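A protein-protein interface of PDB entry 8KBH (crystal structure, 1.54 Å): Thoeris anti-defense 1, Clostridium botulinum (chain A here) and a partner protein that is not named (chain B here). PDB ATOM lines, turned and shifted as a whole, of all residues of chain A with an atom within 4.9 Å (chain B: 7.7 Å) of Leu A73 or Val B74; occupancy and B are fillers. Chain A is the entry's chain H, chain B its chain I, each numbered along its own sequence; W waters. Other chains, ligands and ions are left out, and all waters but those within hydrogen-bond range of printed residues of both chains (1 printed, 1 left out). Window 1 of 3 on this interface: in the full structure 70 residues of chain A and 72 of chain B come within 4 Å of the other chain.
The guanidinium group (NE) of Arg B77 is in salt-bridge range of the side-chain carboxylate (OD2) of Asp A69, at 2.8 Å. OE2 of Glu A74 is in hydrogen-bond range of N of Ile B6, 2.8 Å away.
NH1 of Arg A77 lies within salt-bridge range of OE1 of Glu A74 (2.9 Å). N of Leu B3 lies within hydrogen-bond range of O of Val B15.
Asp A69 touches Val B74. CG2 of Val B74 touches CD1 of Leu A73 (3.6 Å). O of Glu A74 touches CD1 of Leu B3 (3.7 Å). Val B15 touches Ile A75. Val A76 touches Leu B71. O of Ala B94 touches CB of Ala A103 (3.7 Å). Ala A103 touches His B97. Val B98 touches Ala A103. CB of Leu A104 touches CD1 of Ile B6, at 3.5 Å. Val B74 touches Met A107.
Of chain B, only Val B74 (3.6 Å) comes within 4 Å of Leu A73. Of the printed residues of chain B, Val A76 touches Asp B67 (3.7 Å) and Leu B71 (3.6 Å). Printed residues of chain A within 4 Å of Ile B6: Glu A74, Arg A77 and Leu A104. Ile B73 touches none of the printed residues of chain A. Of chain A, only Asp A69, Leu A73 and Met A107 come within 4 Å of Val B74. Phe B81 touches none of the printed residues of chain A. The nearest residue of chain A that does not touch Val B74 is Leu A72 (4.3 Å). The nearest printed residue of chain B that does not touch Arg A77 is Asp B67 (6.0 Å).
Hydrophobic or aromatic side chains of chain B within 4 Å of the printed part of chain A: Leu B3, Ile B6, Val B15, Leu B71, Val B74, Ala B94, His B97, Val B98 and Ala B101. Hydrophobic or aromatic side chains of chain A that line the printed part of chain B: Leu A73, Ile A75, Val A76, Val A100, Ala A103, Leu A104 and Met A107. Among the printed residues, 15 pairs touch across the chains. Among the printed residues, Asp or Glu carboxylates within 4 Å of a Lys or Arg side-chain nitrogen of the other chain: Asp A69 with Arg B77.
Water W1 bridges OE2 of Glu A74 (2.7 Å) and N of Ile B6 (3.4 Å).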
ATOM      1  N   ASP A  69      -4.108 -24.664 -25.487  1.00  0.00           N
ATOM      2  CA  ASP A  69      -3.540 -25.814 -24.778  1.00  0.00           C
ATOM      3  C   ASP A  69      -4.295 -26.100 -23.487  1.00  0.00           C
ATOM      4  O   ASP A  69      -4.444 -27.267 -23.079  1.00  0.00           O
ATOM      5  CB  ASP A  69      -2.074 -25.544 -24.478  1.00  0.00           C
ATOM      6  CG  ASP A  69      -1.296 -25.197 -25.722  1.00  0.00           C
ATOM      7  OD1 ASP A  69      -1.404 -24.029 -26.148  1.00  0.00           O
ATOM      8  OD2 ASP A  69      -0.608 -26.067 -26.285  1.00  0.00           O
ATOM      9  N   SER A  70      -4.768 -25.040 -22.826  1.00  0.00           N
ATOM     10  CA  SER A  70      -5.482 -25.209 -21.567  1.00  0.00           C
ATOM     11  C   SER A  70      -6.774 -25.992 -21.763  1.00  0.00           C
ATOM     12  O   SER A  70      -7.206 -26.683 -20.840  1.00  0.00           O
ATOM     13  CB  SER A  70      -5.751 -23.848 -20.906  1.00  0.00           C
ATOM     14  OG  SER A  70      -6.586 -23.007 -21.695  1.00  0.00           O
ATOM     15  N   ASP A  71      -7.398 -25.910 -22.949  1.00  0.00           N
ATOM     16  CA  ASP A  71      -8.579 -26.735 -23.225  1.00  0.00           C
ATOM     17  C   ASP A  71      -8.233 -28.218 -23.137  1.00  0.00           C
ATOM     18  O   ASP A  71      -8.966 -29.019 -22.531  1.00  0.00           O
ATOM     19  CB  ASP A  71      -9.163 -26.439 -24.617  1.00  0.00           C
ATOM     20  CG  ASP A  71      -9.541 -24.980 -24.832  1.00  0.00           C
ATOM     21  OD1 ASP A  71      -9.950 -24.316 -23.861  1.00  0.00           O
ATOM     22  OD2 ASP A  71      -9.518 -24.532 -26.009  1.00  0.00           O
ATOM     23  N   LEU A  72      -7.113 -28.604 -23.747  1.00  0.00           N
ATOM     24  CA  LEU A  72      -6.708 -30.002 -23.706  1.00  0.00           C
ATOM     25  C   LEU A  72      -6.372 -30.428 -22.277  1.00  0.00           C
ATOM     26  O   LEU A  72      -6.793 -31.503 -21.821  1.00  0.00           O
ATOM     27  CB  LEU A  72      -5.534 -30.231 -24.657  1.00  0.00           C
ATOM     28  CG  LEU A  72      -5.697 -29.766 -26.119  1.00  0.00           C
ATOM     29  CD1 LEU A  72      -4.547 -30.283 -26.969  1.00  0.00           C
ATOM     30  CD2 LEU A  72      -7.055 -30.150 -26.732  1.00  0.00           C
ATOM     31  N   LEU A  73      -5.665 -29.573 -21.536  1.00  0.00           N
ATOM     32  CA  LEU A  73      -5.386 -29.906 -20.139  1.00  0.00           C
ATOM     33  C   LEU A  73      -6.649 -29.978 -19.289  1.00  0.00           C
ATOM     34  O   LEU A  73      -6.721 -30.817 -18.390  1.00  0.00           O
ATOM     35  CB  LEU A  73      -4.393 -28.910 -19.527  1.00  0.00           C
ATOM     36  CG  LEU A  73      -2.937 -29.375 -19.606  1.00  0.00           C
ATOM     37  CD1 LEU A  73      -2.495 -29.516 -21.025  1.00  0.00           C
ATOM     38  CD2 LEU A  73      -2.035 -28.413 -18.840  1.00  0.00           C
ATOM     39  N   GLU A  74      -7.653 -29.133 -19.539  1.00  0.00           N
ATOM     40  CA  GLU A  74      -8.886 -29.235 -18.767  1.00  0.00           C
ATOM     41  C   GLU A  74      -9.608 -30.547 -19.064  1.00  0.00           C
ATOM     42  O   GLU A  74     -10.221 -31.146 -18.166  1.00  0.00           O
ATOM     43  CB  GLU A  74      -9.791 -28.030 -19.039  1.00  0.00           C
ATOM     44  CG  GLU A  74      -9.273 -26.716 -18.450  1.00  0.00           C
ATOM     45  CD  GLU A  74      -9.412 -26.608 -16.931  1.00  0.00           C
ATOM     46  OE1 GLU A  74     -10.070 -27.477 -16.317  1.00  0.00           O
ATOM     47  OE2 GLU A  74      -8.858 -25.645 -16.339  1.00  0.00           O
ATOM     48  N   ILE A  75      -9.541 -31.018 -20.312  1.00  0.00           N
ATOM     49  CA  ILE A  75     -10.142 -32.316 -20.631  1.00  0.00           C
ATOM     50  C   ILE A  75      -9.441 -33.425 -19.852  1.00  0.00           C
ATOM     51  O   ILE A  75     -10.082 -34.294 -19.234  1.00  0.00           O
ATOM     52  CB  ILE A  75     -10.081 -32.575 -22.145  1.00  0.00           C
ATOM     53  CG1 ILE A  75     -11.025 -31.619 -22.884  1.00  0.00           C
ATOM     54  CG2 ILE A  75     -10.464 -34.025 -22.446  1.00  0.00           C
ATOM     55  CD1 ILE A  75     -10.783 -31.560 -24.386  1.00  0.00           C
ATOM     56  N   VAL A  76      -8.107 -33.406 -19.868  1.00  0.00           N
ATOM     57  CA  VAL A  76      -7.341 -34.416 -19.136  1.00  0.00           C
ATOM     58  C   VAL A  76      -7.624 -34.337 -17.636  1.00  0.00           C
ATOM     59  O   VAL A  76      -7.821 -35.359 -16.972  1.00  0.00           O
ATOM     60  CB  VAL A  76      -5.842 -34.280 -19.464  1.00  0.00           C
ATOM     61  CG1 VAL A  76      -5.014 -35.195 -18.579  1.00  0.00           C
ATOM     62  CG2 VAL A  76      -5.606 -34.613 -20.939  1.00  0.00           C
ATOM     63  N   ARG A  77      -7.650 -33.125 -17.081  1.00  0.00           N
ATOM     64  CA  ARG A  77      -7.959 -32.929 -15.668  1.00  0.00           C
ATOM     65  C   ARG A  77      -9.305 -33.544 -15.296  1.00  0.00           C
ATOM     66  O   ARG A  77      -9.417 -34.234 -14.275  1.00  0.00           O
ATOM     67  CB  ARG A  77      -7.941 -31.425 -15.374  1.00  0.00           C
ATOM     68  CG  ARG A  77      -8.591 -31.012 -14.071  1.00  0.00           C
ATOM     69  CD  ARG A  77      -8.640 -29.483 -13.919  1.00  0.00           C
ATOM     70  NE  ARG A  77      -9.200 -29.093 -12.631  1.00  0.00           N
ATOM     71  CZ  ARG A  77     -10.149 -28.178 -12.453  1.00  0.00           C
ATOM     72  NH1 ARG A  77     -10.662 -27.531 -13.486  1.00  0.00           N
ATOM     73  NH2 ARG A  77     -10.577 -27.913 -11.228  1.00  0.00           N
ATOM     74  N   VAL A 100      -1.011 -31.736 -13.620  1.00  0.00           N
ATOM     75  CA  VAL A 100      -1.845 -31.119 -14.655  1.00  0.00           C
ATOM     76  C   VAL A 100      -2.496 -29.846 -14.127  1.00  0.00           C
ATOM     77  O   VAL A 100      -2.540 -28.821 -14.819  1.00  0.00           O
ATOM     78  CB  VAL A 100      -2.905 -32.113 -15.177  1.00  0.00           C
ATOM     79  CG1 VAL A 100      -4.015 -31.369 -15.974  1.00  0.00           C
ATOM     80  CG2 VAL A 100      -2.244 -33.157 -16.035  1.00  0.00           C
ATOM     81  N   ALA A 103       0.047 -27.100 -13.785  1.00  0.00           N
ATOM     82  CA  ALA A 103       0.353 -26.554 -15.103  1.00  0.00           C
ATOM     83  C   ALA A 103      -0.741 -25.608 -15.569  1.00  0.00           C
ATOM     84  O   ALA A 103      -0.453 -24.547 -16.134  1.00  0.00           O
ATOM     85  CB  ALA A 103       0.527 -27.675 -16.128  1.00  0.00           C
ATOM     86  N   LEU A 104      -2.005 -25.987 -15.367  1.00  0.00           N
ATOM     87  CA  LEU A 104      -3.102 -25.100 -15.752  1.00  0.00           C
ATOM     88  C   LEU A 104      -3.063 -23.809 -14.962  1.00  0.00           C
ATOM     89  O   LEU A 104      -3.335 -22.729 -15.505  1.00  0.00           O
ATOM     90  CB  LEU A 104      -4.449 -25.763 -15.524  1.00  0.00           C
ATOM     91  CG  LEU A 104      -4.941 -26.682 -16.621  1.00  0.00           C
ATOM     92  CD1 LEU A 104      -5.947 -27.641 -16.025  1.00  0.00           C
ATOM     93  CD2 LEU A 104      -5.541 -25.867 -17.753  1.00  0.00           C
ATOM     94  N   MET A 107      -0.485 -21.712 -16.573  1.00  0.00           N
ATOM     95  CA  MET A 107      -1.008 -21.140 -17.816  1.00  0.00           C
ATOM     96  C   MET A 107      -1.957 -19.985 -17.515  1.00  0.00           C
ATOM     97  O   MET A 107      -2.016 -18.985 -18.253  1.00  0.00           O
ATOM     98  CB  MET A 107      -1.728 -22.215 -18.626  1.00  0.00           C
ATOM     99  CG  MET A 107      -0.844 -23.276 -19.195  1.00  0.00           C
ATOM    100  SD  MET A 107      -1.823 -24.557 -20.017  1.00  0.00           S
ATOM    101  CE  MET A 107      -0.524 -25.525 -20.762  1.00  0.00           C
ATOM    102  N   LEU B   3     -17.376 -27.819 -18.436  1.00  0.00           N
ATOM    103  CA  LEU B   3     -16.287 -27.935 -17.477  1.00  0.00           C
ATOM    104  C   LEU B   3     -16.064 -26.625 -16.737  1.00  0.00           C
ATOM    105  O   LEU B   3     -15.928 -25.565 -17.349  1.00  0.00           O
ATOM    106  CB  LEU B   3     -14.995 -28.364 -18.171  1.00  0.00           C
ATOM    107  CG  LEU B   3     -14.988 -29.717 -18.879  1.00  0.00           C
ATOM    108  CD1 LEU B   3     -13.562 -30.081 -19.242  1.00  0.00           C
ATOM    109  CD2 LEU B   3     -15.620 -30.784 -18.001  1.00  0.00           C
ATOM    110  N   ILE B   6      -9.986 -23.751 -14.534  1.00  0.00           N
ATOM    111  CA  ILE B   6      -9.165 -22.905 -13.673  1.00  0.00           C
ATOM    112  C   ILE B   6      -9.124 -21.475 -14.194  1.00  0.00           C
ATOM    113  O   ILE B   6      -9.143 -20.521 -13.410  1.00  0.00           O
ATOM    114  CB  ILE B   6      -7.753 -23.504 -13.486  1.00  0.00           C
ATOM    115  CG1 ILE B   6      -7.827 -24.762 -12.598  1.00  0.00           C
ATOM    116  CG2 ILE B   6      -6.783 -22.447 -12.955  1.00  0.00           C
ATOM    117  CD1 ILE B   6      -6.740 -25.812 -12.860  1.00  0.00           C
ATOM    118  N   VAL B  15     -15.422 -26.013 -22.869  1.00  0.00           N
ATOM    119  CA  VAL B  15     -15.262 -27.456 -22.986  1.00  0.00           C
ATOM    120  C   VAL B  15     -16.467 -28.135 -22.348  1.00  0.00           C
ATOM    121  O   VAL B  15     -16.914 -27.738 -21.266  1.00  0.00           O
ATOM    122  CB  VAL B  15     -13.957 -27.941 -22.322  1.00  0.00           C
ATOM    123  CG1 VAL B  15     -13.678 -29.367 -22.731  1.00  0.00           C
ATOM    124  CG2 VAL B  15     -12.786 -27.045 -22.700  1.00  0.00           C
ATOM    125  N   ASP B  67      -4.685 -39.641 -23.042  1.00  0.00           N
ATOM    126  CA  ASP B  67      -4.371 -38.322 -22.481  1.00  0.00           C
ATOM    127  C   ASP B  67      -2.906 -37.933 -22.683  1.00  0.00           C
ATOM    128  O   ASP B  67      -2.592 -36.748 -22.873  1.00  0.00           O
ATOM    129  CB  ASP B  67      -4.739 -38.294 -21.003  1.00  0.00           C
ATOM    130  CG  ASP B  67      -6.125 -38.840 -20.760  1.00  0.00           C
ATOM    131  OD1 ASP B  67      -6.298 -40.075 -20.890  1.00  0.00           O
ATOM    132  OD2 ASP B  67      -7.035 -38.036 -20.481  1.00  0.00           O
ATOM    133  N   SER B  68      -1.989 -38.904 -22.618  1.00  0.00           N
ATOM    134  CA  SER B  68      -0.582 -38.575 -22.813  1.00  0.00           C
ATOM    135  C   SER B  68      -0.320 -37.997 -24.202  1.00  0.00           C
ATOM    136  O   SER B  68       0.601 -37.191 -24.354  1.00  0.00           O
ATOM    137  CB  SER B  68       0.302 -39.800 -22.550  1.00  0.00           C
ATOM    138  OG  SER B  68      -0.016 -40.877 -23.415  1.00  0.00           O
ATOM    139  N   ASP B  69      -1.131 -38.366 -25.214  1.00  0.00           N
ATOM    140  CA  ASP B  69      -1.003 -37.763 -26.546  1.00  0.00           C
ATOM    141  C   ASP B  69      -1.237 -36.253 -26.489  1.00  0.00           C
ATOM    142  O   ASP B  69      -0.453 -35.457 -27.039  1.00  0.00           O
ATOM    143  CB  ASP B  69      -2.005 -38.386 -27.531  1.00  0.00           C
ATOM    144  CG  ASP B  69      -1.842 -39.889 -27.690  1.00  0.00           C
ATOM    145  OD1 ASP B  69      -0.698 -40.391 -27.667  1.00  0.00           O
ATOM    146  OD2 ASP B  69      -2.883 -40.565 -27.872  1.00  0.00           O
ATOM    147  N   LEU B  70      -2.331 -35.845 -25.834  1.00  0.00           N
ATOM    148  CA  LEU B  70      -2.630 -34.424 -25.689  1.00  0.00           C
ATOM    149  C   LEU B  70      -1.545 -33.711 -24.891  1.00  0.00           C
ATOM    150  O   LEU B  70      -1.116 -32.605 -25.259  1.00  0.00           O
ATOM    151  CB  LEU B  70      -4.005 -34.228 -25.038  1.00  0.00           C
ATOM    152  CG  LEU B  70      -5.233 -34.960 -25.613  1.00  0.00           C
ATOM    153  CD1 LEU B  70      -6.496 -34.513 -24.886  1.00  0.00           C
ATOM    154  CD2 LEU B  70      -5.344 -34.683 -27.105  1.00  0.00           C
ATOM    155  N   LEU B  71      -1.064 -34.337 -23.812  1.00  0.00           N
ATOM    156  CA  LEU B  71      -0.013 -33.692 -23.031  1.00  0.00           C
ATOM    157  C   LEU B  71       1.298 -33.599 -23.808  1.00  0.00           C
ATOM    158  O   LEU B  71       2.044 -32.635 -23.636  1.00  0.00           O
ATOM    159  CB  LEU B  71       0.201 -34.424 -21.703  1.00  0.00           C
ATOM    160  CG  LEU B  71      -0.620 -33.896 -20.522  1.00  0.00           C
ATOM    161  CD1 LEU B  71      -2.092 -34.137 -20.732  1.00  0.00           C
ATOM    162  CD2 LEU B  71      -0.153 -34.532 -19.221  1.00  0.00           C
ATOM    163  N   GLU B  72       1.596 -34.571 -24.676  1.00  0.00           N
ATOM    164  CA  GLU B  72       2.804 -34.463 -25.483  1.00  0.00           C
ATOM    165  C   GLU B  72       2.687 -33.329 -26.494  1.00  0.00           C
ATOM    166  O   GLU B  72       3.659 -32.602 -26.735  1.00  0.00           O
ATOM    167  CB  GLU B  72       3.093 -35.794 -26.177  1.00  0.00           C
ATOM    168  CG  GLU B  72       3.558 -36.876 -25.219  1.00  0.00           C
ATOM    169  CD  GLU B  72       5.023 -36.748 -24.853  1.00  0.00           C
ATOM    170  OE1 GLU B  72       5.699 -35.832 -25.376  1.00  0.00           O
ATOM    171  OE2 GLU B  72       5.501 -37.564 -24.033  1.00  0.00           O
ATOM    172  N   ILE B  73       1.496 -33.139 -27.068  1.00  0.00           N
ATOM    173  CA  ILE B  73       1.294 -31.990 -27.952  1.00  0.00           C
ATOM    174  C   ILE B  73       1.543 -30.681 -27.204  1.00  0.00           C
ATOM    175  O   ILE B  73       2.247 -29.785 -27.697  1.00  0.00           O
ATOM    176  CB  ILE B  73      -0.113 -32.032 -28.571  1.00  0.00           C
ATOM    177  CG1 ILE B  73      -0.200 -33.204 -29.554  1.00  0.00           C
ATOM    178  CG2 ILE B  73      -0.443 -30.698 -29.249  1.00  0.00           C
ATOM    179  CD1 ILE B  73      -1.594 -33.487 -30.081  1.00  0.00           C
ATOM    180  N   VAL B  74       0.967 -30.549 -26.002  1.00  0.00           N
ATOM    181  CA  VAL B  74       1.143 -29.312 -25.236  1.00  0.00           C
ATOM    182  C   VAL B  74       2.607 -29.118 -24.849  1.00  0.00           C
ATOM    183  O   VAL B  74       3.133 -28.000 -24.884  1.00  0.00           O
ATOM    184  CB  VAL B  74       0.229 -29.304 -23.998  1.00  0.00           C
ATOM    185  CG1 VAL B  74       0.585 -28.139 -23.081  1.00  0.00           C
ATOM    186  CG2 VAL B  74      -1.225 -29.223 -24.417  1.00  0.00           C
ATOM    187  N   ARG B  75       3.272 -30.200 -24.450  1.00  0.00           N
ATOM    188  CA  ARG B  75       4.705 -30.185 -24.162  1.00  0.00           C
ATOM    189  C   ARG B  75       5.508 -29.658 -25.345  1.00  0.00           C
ATOM    190  O   ARG B  75       6.375 -28.788 -25.190  1.00  0.00           O
ATOM    191  CB  ARG B  75       5.135 -31.609 -23.811  1.00  0.00           C
ATOM    192  CG  ARG B  75       6.595 -31.786 -23.549  1.00  0.00           C
ATOM    193  CD  ARG B  75       6.961 -33.268 -23.497  1.00  0.00           C
ATOM    194  NE  ARG B  75       8.395 -33.433 -23.317  1.00  0.00           N
ATOM    195  CZ  ARG B  75       9.133 -34.397 -23.861  1.00  0.00           C
ATOM    196  NH1 ARG B  75       8.590 -35.328 -24.641  1.00  0.00           N
ATOM    197  NH2 ARG B  75      10.433 -34.425 -23.612  1.00  0.00           N
ATOM    198  N   ASP B  76       5.232 -30.185 -26.535  1.00  0.00           N
ATOM    199  CA  ASP B  76       5.973 -29.779 -27.725  1.00  0.00           C
ATOM    200  C   ASP B  76       5.751 -28.306 -28.017  1.00  0.00           C
ATOM    201  O   ASP B  76       6.700 -27.566 -28.321  1.00  0.00           O
ATOM    202  CB  ASP B  76       5.536 -30.645 -28.906  1.00  0.00           C
ATOM    203  CG  ASP B  76       6.406 -30.457 -30.122  1.00  0.00           C
ATOM    204  OD1 ASP B  76       7.610 -30.787 -30.054  1.00  0.00           O
ATOM    205  OD2 ASP B  76       5.878 -29.982 -31.153  1.00  0.00           O
ATOM    206  N   ARG B  77       4.500 -27.858 -27.909  1.00  0.00           N
ATOM    207  CA  ARG B  77       4.215 -26.449 -28.147  1.00  0.00           C
ATOM    208  C   ARG B  77       4.908 -25.567 -27.120  1.00  0.00           C
ATOM    209  O   ARG B  77       5.443 -24.511 -27.468  1.00  0.00           O
ATOM    210  CB  ARG B  77       2.707 -26.213 -28.170  1.00  0.00           C
ATOM    211  CG  ARG B  77       2.101 -26.609 -29.512  1.00  0.00           C
ATOM    212  CD  ARG B  77       0.591 -26.645 -29.528  1.00  0.00           C
ATOM    213  NE  ARG B  77       0.017 -25.453 -28.921  1.00  0.00           N
ATOM    214  CZ  ARG B  77      -0.205 -24.316 -29.568  1.00  0.00           C
ATOM    215  NH1 ARG B  77       0.111 -24.189 -30.854  1.00  0.00           N
ATOM    216  NH2 ARG B  77      -0.733 -23.301 -28.915  1.00  0.00           N
ATOM    217  N   LEU B  78       4.950 -25.998 -25.858  1.00  0.00           N
ATOM    218  CA  LEU B  78       5.598 -25.177 -24.844  1.00  0.00           C
ATOM    219  C   LEU B  78       7.100 -25.112 -25.064  1.00  0.00           C
ATOM    220  O   LEU B  78       7.723 -24.064 -24.847  1.00  0.00           O
ATOM    221  CB  LEU B  78       5.278 -25.701 -23.445  1.00  0.00           C
ATOM    222  CG  LEU B  78       3.865 -25.416 -22.942  1.00  0.00           C
ATOM    223  CD1 LEU B  78       3.601 -26.119 -21.593  1.00  0.00           C
ATOM    224  CD2 LEU B  78       3.627 -23.913 -22.807  1.00  0.00           C
ATOM    225  N   LYS B  79       7.698 -26.218 -25.505  1.00  0.00           N
ATOM    226  CA  LYS B  79       9.116 -26.185 -25.842  1.00  0.00           C
ATOM    227  C   LYS B  79       9.376 -25.221 -26.990  1.00  0.00           C
ATOM    228  O   LYS B  79      10.340 -24.443 -26.951  1.00  0.00           O
ATOM    229  CB  LYS B  79       9.600 -27.590 -26.177  1.00  0.00           C
ATOM    230  CG  LYS B  79       9.403 -28.565 -25.033  1.00  0.00           C
ATOM    231  CD  LYS B  79       9.757 -29.971 -25.429  1.00  0.00           C
ATOM    232  CE  LYS B  79      11.158 -30.044 -25.969  1.00  0.00           C
ATOM    233  NZ  LYS B  79      11.447 -31.440 -26.409  1.00  0.00           N
ATOM    234  N   SER B  80       8.510 -25.235 -28.007  1.00  0.00           N
ATOM    235  CA  SER B  80       8.681 -24.300 -29.120  1.00  0.00           C
ATOM    236  C   SER B  80       8.518 -22.850 -28.661  1.00  0.00           C
ATOM    237  O   SER B  80       9.257 -21.961 -29.103  1.00  0.00           O
ATOM    238  CB  SER B  80       7.696 -24.630 -30.240  1.00  0.00           C
ATOM    239  OG  SER B  80       7.901 -25.938 -30.758  1.00  0.00           O
ATOM    240  N   PHE B  81       7.574 -22.590 -27.755  1.00  0.00           N
ATOM    241  CA  PHE B  81       7.395 -21.223 -27.282  1.00  0.00           C
ATOM    242  C   PHE B  81       8.582 -20.775 -26.445  1.00  0.00           C
ATOM    243  O   PHE B  81       8.982 -19.606 -26.509  1.00  0.00           O
ATOM    244  CB  PHE B  81       6.103 -21.096 -26.472  1.00  0.00           C
ATOM    245  CG  PHE B  81       4.858 -21.162 -27.306  1.00  0.00           C
ATOM    246  CD1 PHE B  81       4.803 -20.546 -28.545  1.00  0.00           C
ATOM    247  CD2 PHE B  81       3.750 -21.862 -26.861  1.00  0.00           C
ATOM    248  CE1 PHE B  81       3.672 -20.627 -29.318  1.00  0.00           C
ATOM    249  CE2 PHE B  81       2.608 -21.939 -27.632  1.00  0.00           C
ATOM    250  CZ  PHE B  81       2.570 -21.317 -28.862  1.00  0.00           C
ATOM    251  N   ALA B  94       4.883 -24.239 -16.295  1.00  0.00           N
ATOM    252  CA  ALA B  94       3.850 -25.081 -16.887  1.00  0.00           C
ATOM    253  C   ALA B  94       4.458 -26.262 -17.625  1.00  0.00           C
ATOM    254  O   ALA B  94       3.975 -27.388 -17.497  1.00  0.00           O
ATOM    255  CB  ALA B  94       2.966 -24.255 -17.819  1.00  0.00           C
ATOM    256  N   LEU B  95       5.512 -26.024 -18.409  1.00  0.00           N
ATOM    257  CA  LEU B  95       6.161 -27.099 -19.149  1.00  0.00           C
ATOM    258  C   LEU B  95       6.722 -28.168 -18.219  1.00  0.00           C
ATOM    259  O   LEU B  95       6.556 -29.369 -18.475  1.00  0.00           O
ATOM    260  CB  LEU B  95       7.271 -26.527 -20.030  1.00  0.00           C
ATOM    261  CG  LEU B  95       8.140 -27.596 -20.687  1.00  0.00           C
ATOM    262  CD1 LEU B  95       7.386 -28.505 -21.696  1.00  0.00           C
ATOM    263  CD2 LEU B  95       9.288 -26.892 -21.368  1.00  0.00           C
ATOM    264  N   HIS B  97       5.739 -28.900 -15.194  1.00  0.00           N
ATOM    265  CA  HIS B  97       4.597 -29.630 -14.625  1.00  0.00           C
ATOM    266  C   HIS B  97       3.972 -30.596 -15.637  1.00  0.00           C
ATOM    267  O   HIS B  97       3.628 -31.730 -15.278  1.00  0.00           O
ATOM    268  CB  HIS B  97       3.543 -28.656 -14.082  1.00  0.00           C
ATOM    269  CG  HIS B  97       3.840 -28.145 -12.703  1.00  0.00           C
ATOM    270  ND1 HIS B  97       3.983 -28.977 -11.612  1.00  0.00           N
ATOM    271  CD2 HIS B  97       4.030 -26.887 -12.238  1.00  0.00           C
ATOM    272  CE1 HIS B  97       4.239 -28.256 -10.534  1.00  0.00           C
ATOM    273  NE2 HIS B  97       4.273 -26.985 -10.885  1.00  0.00           N
ATOM    274  N   VAL B  98       3.803 -30.175 -16.894  1.00  0.00           N
ATOM    275  CA  VAL B  98       3.306 -31.080 -17.940  1.00  0.00           C
ATOM    276  C   VAL B  98       4.237 -32.282 -18.106  1.00  0.00           C
ATOM    277  O   VAL B  98       3.783 -33.424 -18.243  1.00  0.00           O
ATOM    278  CB  VAL B  98       3.127 -30.330 -19.273  1.00  0.00           C
ATOM    279  CG1 VAL B  98       2.965 -31.347 -20.434  1.00  0.00           C
ATOM    280  CG2 VAL B  98       1.948 -29.399 -19.212  1.00  0.00           C
ATOM    281  N   ALA B 101       3.760 -34.604 -15.162  1.00  0.00           N
ATOM    282  CA  ALA B 101       2.519 -35.354 -15.395  1.00  0.00           C
ATOM    283  C   ALA B 101       2.730 -36.495 -16.393  1.00  0.00           C
ATOM    284  O   ALA B 101       2.248 -37.613 -16.186  1.00  0.00           O
ATOM    285  CB  ALA B 101       1.409 -34.415 -15.878  1.00  0.00           C
ATOM    286  N   LEU B 102       3.450 -36.233 -17.487  1.00  0.00           N
ATOM    287  CA  LEU B 102       3.677 -37.297 -18.466  1.00  0.00           C
ATOM    288  C   LEU B 102       4.521 -38.416 -17.876  1.00  0.00           C
ATOM    289  O   LEU B 102       4.327 -39.596 -18.201  1.00  0.00           O
ATOM    290  CB  LEU B 102       4.350 -36.739 -19.719  1.00  0.00           C
ATOM    291  CG  LEU B 102       3.391 -36.056 -20.675  1.00  0.00           C
ATOM    292  CD1 LEU B 102       4.144 -35.106 -21.606  1.00  0.00           C
ATOM    293  CD2 LEU B 102       2.660 -37.127 -21.471  1.00  0.00           C
HETATM  294  O   HOH W   1      -8.125 -23.305 -17.366  1.00  0.00           O
